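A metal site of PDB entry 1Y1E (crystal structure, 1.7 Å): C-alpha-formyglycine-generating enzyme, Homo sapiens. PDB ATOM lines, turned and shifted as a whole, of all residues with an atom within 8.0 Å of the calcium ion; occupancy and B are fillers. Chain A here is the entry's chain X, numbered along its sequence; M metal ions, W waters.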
ATOM      1  N   HIS A 184      -7.343  15.492  -3.620  1.00  0.00           N
ATOM      2  CA  HIS A 184      -7.112  16.314  -2.433  1.00  0.00           C
ATOM      3  C   HIS A 184      -7.252  17.797  -2.782  1.00  0.00           C
ATOM      4  O   HIS A 184      -6.670  18.298  -3.765  1.00  0.00           O
ATOM      5  CB  HIS A 184      -5.764  15.998  -1.786  1.00  0.00           C
ATOM      6  CG  HIS A 184      -5.743  14.703  -1.038  1.00  0.00           C
ATOM      7  ND1 HIS A 184      -6.321  14.552   0.202  1.00  0.00           N
ATOM      8  CD2 HIS A 184      -5.262  13.484  -1.380  1.00  0.00           C
ATOM      9  CE1 HIS A 184      -6.174  13.297   0.598  1.00  0.00           C
ATOM     10  NE2 HIS A 184      -5.546  12.628  -0.347  1.00  0.00           N
ATOM     11  N   ALA A 186      -7.058  20.342  -0.084  1.00  0.00           N
ATOM     12  CA  ALA A 186      -6.564  21.099   1.068  1.00  0.00           C
ATOM     13  C   ALA A 186      -5.523  20.267   1.808  1.00  0.00           C
ATOM     14  O   ALA A 186      -5.547  19.035   1.746  1.00  0.00           O
ATOM     15  CB  ALA A 186      -7.689  21.445   2.041  1.00  0.00           C
ATOM     16  N   ASN A 187      -4.629  20.960   2.502  1.00  0.00           N
ATOM     17  CA  ASN A 187      -3.542  20.322   3.224  1.00  0.00           C
ATOM     18  C   ASN A 187      -3.977  20.128   4.660  1.00  0.00           C
ATOM     19  O   ASN A 187      -3.918  21.067   5.467  1.00  0.00           O
ATOM     20  CB  ASN A 187      -2.278  21.155   3.112  1.00  0.00           C
ATOM     21  CG  ASN A 187      -1.119  20.580   3.911  1.00  0.00           C
ATOM     22  OD1 ASN A 187      -1.114  19.376   4.214  1.00  0.00           O
ATOM     23  ND2 ASN A 187      -0.162  21.435   4.281  1.00  0.00           N
ATOM     24  N   ILE A 188      -4.484  18.925   4.940  1.00  0.00           N
ATOM     25  CA  ILE A 188      -4.799  18.498   6.320  1.00  0.00           C
ATOM     26  C   ILE A 188      -3.991  17.222   6.693  1.00  0.00           C
ATOM     27  O   ILE A 188      -2.928  16.932   6.112  1.00  0.00           O
ATOM     28  CB  ILE A 188      -6.343  18.382   6.537  1.00  0.00           C
ATOM     29  CG1 ILE A 188      -6.972  17.414   5.534  1.00  0.00           C
ATOM     30  CG2 ILE A 188      -7.003  19.761   6.491  1.00  0.00           C
ATOM     31  CD1 ILE A 188      -8.380  16.975   5.927  1.00  0.00           C
ATOM     32  N   TRP A 189      -4.473  16.469   7.677  1.00  0.00           N
ATOM     33  CA  TRP A 189      -3.772  15.274   8.151  1.00  0.00           C
ATOM     34  C   TRP A 189      -4.409  14.034   7.541  1.00  0.00           C
ATOM     35  O   TRP A 189      -5.629  13.942   7.473  1.00  0.00           O
ATOM     36  CB  TRP A 189      -3.913  15.205   9.649  1.00  0.00           C
ATOM     37  CG  TRP A 189      -3.128  14.118  10.379  1.00  0.00           C
ATOM     38  CD1 TRP A 189      -3.460  12.786  10.499  1.00  0.00           C
ATOM     39  CD2 TRP A 189      -1.934  14.303  11.108  1.00  0.00           C
ATOM     40  NE1 TRP A 189      -2.508  12.136  11.271  1.00  0.00           N
ATOM     41  CE2 TRP A 189      -1.565  13.046  11.666  1.00  0.00           C
ATOM     42  CE3 TRP A 189      -1.110  15.417  11.355  1.00  0.00           C
ATOM     43  CZ2 TRP A 189      -0.398  12.867  12.420  1.00  0.00           C
ATOM     44  CZ3 TRP A 189       0.045  15.235  12.124  1.00  0.00           C
ATOM     45  CH2 TRP A 189       0.375  13.989  12.669  1.00  0.00           C
ATOM     46  N   GLN A 190      -3.600  13.088   7.088  1.00  0.00           N
ATOM     47  CA  GLN A 190      -4.077  11.734   6.837  1.00  0.00           C
ATOM     48  C   GLN A 190      -3.268  10.792   7.712  1.00  0.00           C
ATOM     49  O   GLN A 190      -2.113  11.049   7.963  1.00  0.00           O
ATOM     50  CB  GLN A 190      -3.952  11.347   5.366  1.00  0.00           C
ATOM     51  CG  GLN A 190      -4.777  12.241   4.433  1.00  0.00           C
ATOM     52  CD  GLN A 190      -4.007  13.482   4.013  1.00  0.00           C
ATOM     53  OE1 GLN A 190      -2.783  13.429   3.794  1.00  0.00           O
ATOM     54  NE2 GLN A 190      -4.726  14.613   3.890  1.00  0.00           N
ATOM     55  N   ASN A 197       1.410  10.786  10.330  1.00  0.00           N
ATOM     56  CA  ASN A 197       0.882  11.567   9.216  1.00  0.00           C
ATOM     57  C   ASN A 197       1.452  10.927   7.959  1.00  0.00           C
ATOM     58  O   ASN A 197       2.664  10.974   7.724  1.00  0.00           O
ATOM     59  CB  ASN A 197       1.290  13.042   9.340  1.00  0.00           C
ATOM     60  CG  ASN A 197       0.581  13.959   8.308  1.00  0.00           C
ATOM     61  OD1 ASN A 197       0.027  13.492   7.304  1.00  0.00           O
ATOM     62  ND2 ASN A 197       0.655  15.254   8.556  1.00  0.00           N
ATOM     63  N   THR A 198       0.578  10.313   7.169  1.00  0.00           N
ATOM     64  CA  THR A 198       1.016   9.574   5.986  1.00  0.00           C
ATOM     65  C   THR A 198       1.551  10.487   4.882  1.00  0.00           C
ATOM     66  O   THR A 198       2.268  10.022   4.003  1.00  0.00           O
ATOM     67  CB  THR A 198      -0.119   8.718   5.398  1.00  0.00           C
ATOM     68  OG1 THR A 198      -1.128   9.564   4.835  1.00  0.00           O
ATOM     69  CG2 THR A 198      -0.738   7.842   6.434  1.00  0.00           C
ATOM     70  N   GLY A 199       1.183  11.765   4.917  1.00  0.00           N
ATOM     71  CA  GLY A 199       1.553  12.708   3.875  1.00  0.00           C
ATOM     72  C   GLY A 199       0.906  12.387   2.530  1.00  0.00           C
ATOM     73  O   GLY A 199       1.439  12.737   1.483  1.00  0.00           O
ATOM     74  N   GLU A 200      -0.250  11.728   2.565  1.00  0.00           N
ATOM     75  CA  GLU A 200      -0.971  11.307   1.361  1.00  0.00           C
ATOM     76  C   GLU A 200      -1.312  12.499   0.460  1.00  0.00           C
ATOM     77  O   GLU A 200      -1.322  12.354  -0.750  1.00  0.00           O
ATOM     78  CB  GLU A 200      -2.254  10.585   1.767  1.00  0.00           C
ATOM     79  CG  GLU A 200      -3.136  10.087   0.643  1.00  0.00           C
ATOM     80  CD  GLU A 200      -4.514   9.705   1.156  1.00  0.00           C
ATOM     81  OE1 GLU A 200      -4.584   9.144   2.276  1.00  0.00           O
ATOM     82  OE2 GLU A 200      -5.520  10.013   0.482  1.00  0.00           O
ATOM     83  N   ASP A 201      -1.601  13.657   1.056  1.00  0.00           N
ATOM     84  CA  ASP A 201      -2.022  14.822   0.255  1.00  0.00           C
ATOM     85  C   ASP A 201      -0.822  15.581  -0.292  1.00  0.00           C
ATOM     86  O   ASP A 201      -0.970  16.552  -1.005  1.00  0.00           O
ATOM     87  CB  ASP A 201      -2.928  15.757   1.048  1.00  0.00           C
ATOM     88  CG  ASP A 201      -2.249  16.364   2.257  1.00  0.00           C
ATOM     89  OD1 ASP A 201      -0.988  16.312   2.378  1.00  0.00           O
ATOM     90  OD2 ASP A 201      -2.990  16.881   3.103  1.00  0.00           O
ATOM     91  N   GLY A 202       0.374  15.082   0.047  1.00  0.00           N
ATOM     92  CA  GLY A 202       1.626  15.548  -0.543  1.00  0.00           C
ATOM     93  C   GLY A 202       2.441  16.453   0.371  1.00  0.00           C
ATOM     94  O   GLY A 202       3.465  16.978  -0.061  1.00  0.00           O
ATOM     95  N   PHE A 203       1.977  16.653   1.610  1.00  0.00           N
ATOM     96  CA  PHE A 203       2.631  17.547   2.593  1.00  0.00           C
ATOM     97  C   PHE A 203       2.361  17.102   4.014  1.00  0.00           C
ATOM     98  O   PHE A 203       1.209  16.968   4.414  1.00  0.00           O
ATOM     99  CB  PHE A 203       2.121  18.986   2.417  1.00  0.00           C
ATOM    100  CG  PHE A 203       2.361  19.518   1.065  1.00  0.00           C
ATOM    101  CD1 PHE A 203       3.585  20.042   0.716  1.00  0.00           C
ATOM    102  CD2 PHE A 203       1.361  19.441   0.097  1.00  0.00           C
ATOM    103  CE1 PHE A 203       3.822  20.485  -0.580  1.00  0.00           C
ATOM    104  CE2 PHE A 203       1.589  19.868  -1.183  1.00  0.00           C
ATOM    105  CZ  PHE A 203       2.814  20.414  -1.528  1.00  0.00           C
ATOM    106  N   GLN A 204       3.406  16.818   4.772  1.00  0.00           N
ATOM    107  CA  GLN A 204       3.231  16.493   6.185  1.00  0.00           C
ATOM    108  C   GLN A 204       3.105  17.779   7.023  1.00  0.00           C
ATOM    109  O   GLN A 204       2.210  17.892   7.869  1.00  0.00           O
ATOM    110  CB  GLN A 204       4.368  15.599   6.657  1.00  0.00           C
ATOM    111  CG  GLN A 204       4.274  14.219   6.004  1.00  0.00           C
ATOM    112  CD  GLN A 204       5.466  13.362   6.335  1.00  0.00           C
ATOM    113  OE1 GLN A 204       6.603  13.769   6.101  1.00  0.00           O
ATOM    114  NE2 GLN A 204       5.208  12.156   6.871  1.00  0.00           N
ATOM    115  N   GLY A 205       4.004  18.724   6.780  1.00  0.00           N
ATOM    116  CA  GLY A 205       3.930  20.046   7.363  1.00  0.00           C
ATOM    117  C   GLY A 205       3.122  20.922   6.426  1.00  0.00           C
ATOM    118  O   GLY A 205       2.217  20.460   5.767  1.00  0.00           O
ATOM    119  N   THR A 206       3.502  22.202   6.343  1.00  0.00           N
ATOM    120  CA  THR A 206       2.842  23.123   5.447  1.00  0.00           C
ATOM    121  C   THR A 206       3.191  22.815   4.004  1.00  0.00           C
ATOM    122  O   THR A 206       4.154  22.090   3.693  1.00  0.00           O
ATOM    123  CB  THR A 206       3.269  24.574   5.719  1.00  0.00           C
ATOM    124  OG1 THR A 206       4.696  24.645   5.645  1.00  0.00           O
ATOM    125  CG2 THR A 206       2.788  25.038   7.094  1.00  0.00           C
ATOM    126  N   ALA A 207       2.353  23.377   3.137  1.00  0.00           N
ATOM    127  CA  ALA A 207       2.575  23.401   1.701  1.00  0.00           C
ATOM    128  C   ALA A 207       2.830  24.839   1.282  1.00  0.00           C
ATOM    129  O   ALA A 207       2.563  25.776   2.051  1.00  0.00           O
ATOM    130  CB  ALA A 207       1.332  22.868   0.983  1.00  0.00           C
ATOM    131  N   PHE A 212      -2.687  23.486  -4.118  1.00  0.00           N
ATOM    132  CA  PHE A 212      -4.084  23.021  -4.084  1.00  0.00           C
ATOM    133  C   PHE A 212      -4.968  23.951  -4.916  1.00  0.00           C
ATOM    134  O   PHE A 212      -4.542  25.060  -5.273  1.00  0.00           O
ATOM    135  CB  PHE A 212      -4.566  22.821  -2.620  1.00  0.00           C
ATOM    136  CG  PHE A 212      -3.853  21.695  -1.938  1.00  0.00           C
ATOM    137  CD1 PHE A 212      -4.174  20.374  -2.270  1.00  0.00           C
ATOM    138  CD2 PHE A 212      -2.826  21.932  -1.045  1.00  0.00           C
ATOM    139  CE1 PHE A 212      -3.476  19.317  -1.710  1.00  0.00           C
ATOM    140  CE2 PHE A 212      -2.119  20.863  -0.468  1.00  0.00           C
ATOM    141  CZ  PHE A 212      -2.454  19.574  -0.805  1.00  0.00           C
ATOM    142  N   ASN A 225      -3.702  23.923   5.812  1.00  0.00           N
ATOM    143  CA  ASN A 225      -2.367  24.518   5.720  1.00  0.00           C
ATOM    144  C   ASN A 225      -2.100  25.305   7.014  1.00  0.00           C
ATOM    145  O   ASN A 225      -1.845  24.674   8.032  1.00  0.00           O
ATOM    146  CB  ASN A 225      -2.174  25.300   4.418  1.00  0.00           C
ATOM    147  CG  ASN A 225      -0.757  25.203   3.881  1.00  0.00           C
ATOM    148  OD1 ASN A 225      -0.095  24.175   4.044  1.00  0.00           O
ATOM    149  ND2 ASN A 225      -0.295  26.256   3.226  1.00  0.00           N
ATOM    150  N   SER A 261      -5.792  23.657   9.933  1.00  0.00           N
ATOM    151  CA  SER A 261      -4.408  23.536   9.542  1.00  0.00           C
ATOM    152  C   SER A 261      -4.037  22.143   8.999  1.00  0.00           C
ATOM    153  O   SER A 261      -4.838  21.217   8.980  1.00  0.00           O
ATOM    154  CB  SER A 261      -3.519  23.832  10.746  1.00  0.00           C
ATOM    155  OG  SER A 261      -3.428  22.736  11.632  1.00  0.00           O
ATOM    156  N   TYR A 262      -2.774  22.028   8.608  1.00  0.00           N
ATOM    157  CA  TYR A 262      -2.186  20.719   8.228  1.00  0.00           C
ATOM    158  C   TYR A 262      -2.259  19.618   9.293  1.00  0.00           C
ATOM    159  O   TYR A 262      -2.005  18.443   8.995  1.00  0.00           O
ATOM    160  CB  TYR A 262      -0.741  20.906   7.776  1.00  0.00           C
ATOM    161  CG  TYR A 262       0.255  21.244   8.853  1.00  0.00           C
ATOM    162  CD1 TYR A 262       0.702  22.554   9.050  1.00  0.00           C
ATOM    163  CD2 TYR A 262       0.801  20.243   9.650  1.00  0.00           C
ATOM    164  CE1 TYR A 262       1.633  22.854  10.046  1.00  0.00           C
ATOM    165  CE2 TYR A 262       1.736  20.529  10.623  1.00  0.00           C
ATOM    166  CZ  TYR A 262       2.155  21.832  10.811  1.00  0.00           C
ATOM    167  OH  TYR A 262       3.079  22.115  11.775  1.00  0.00           O
ATOM    168  N   MET A 263      -2.599  19.988  10.517  1.00  0.00           N
ATOM    169  CA  MET A 263      -2.697  19.019  11.628  1.00  0.00           C
ATOM    170  C   MET A 263      -4.065  18.385  11.751  1.00  0.00           C
ATOM    171  O   MET A 263      -4.200  17.357  12.448  1.00  0.00           O
ATOM    172  CB  MET A 263      -2.360  19.692  12.963  1.00  0.00           C
ATOM    173  CG  MET A 263      -0.890  19.977  13.187  1.00  0.00           C
ATOM    174  SD  MET A 263      -0.564  21.005  14.643  1.00  0.00           S
ATOM    175  CE  MET A 263      -1.150  19.918  15.964  1.00  0.00           C
ATOM    176  N   CYS A 264      -5.082  18.989  11.124  1.00  0.00           N
ATOM    177  CA  CYS A 264      -6.467  18.592  11.392  1.00  0.00           C
ATOM    178  C   CYS A 264      -6.841  17.258  10.756  1.00  0.00           C
ATOM    179  O   CYS A 264      -6.475  16.983   9.632  1.00  0.00           O
ATOM    180  CB  CYS A 264      -7.465  19.682  10.983  1.00  0.00           C
ATOM    181  SG  CYS A 264      -9.097  19.403  11.731  1.00  0.00           S
HETATM  182 CA    CA M   1      -1.154  17.088   4.704  1.00  0.00          CA
HETATM  183  O   HOH W   1      -1.065  14.643   5.148  1.00  0.00           O
HETATM  184  O   HOH W   2      -0.375  17.521   7.005  1.00  0.00           O
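The side-chain amide nitrogen (ND2) of Asn 187 lies close to the backbone NH (N) of Ala 207.
N of Tyr 262 sits close to O of Asn 187.
The side-chain amide nitrogen (ND2) of Asn 187 sits at hydrogen-bond distance from the side-chain amide oxygen (OD1) of Asn 225 (2.8 Å).
The backbone NH (N) of Asp 201 is in hydrogen-bond range of the side-chain amide oxygen (OE1) of Gln 190 (3.0 Å).
ND2 of Asn 187 is in hydrogen-bond range of O of Gly 205 (3.0 Å).
Within 4 Å of the calcium ion: Asn 187, Ile 188, Asp 201 and Phe 203.
The calcium ion is bound by O of Ile 188 (2.3 Å).
OD1 of Asn 187 is bound to the calcium ion, at 2.3 Å.
O of Phe 203 binds the calcium ion, 2.4 Å away.
The side-chain carboxylate (OD2) of Asp 201 binds the calcium ion (2.4 Å).
OD1 of Asp 201 binds the calcium ion (2.5 Å).
Water W2 binds the calcium ion.
The calcium ion is bound by water W1 (2.5 Å).
The calcium ion has seven donor atoms within binding distance.
Water W1 lies within hydrogen-bond range of OE1 of Gln 190 (2.5 Å) and OD1 of Asn 197 (2.7 Å).
Water W2 lies within hydrogen-bond range of the backbone carbonyl oxygen of Tyr 262, the backbone carbonyl oxygen of Gln 204 and the side-chain amide nitrogen of Asn 197.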
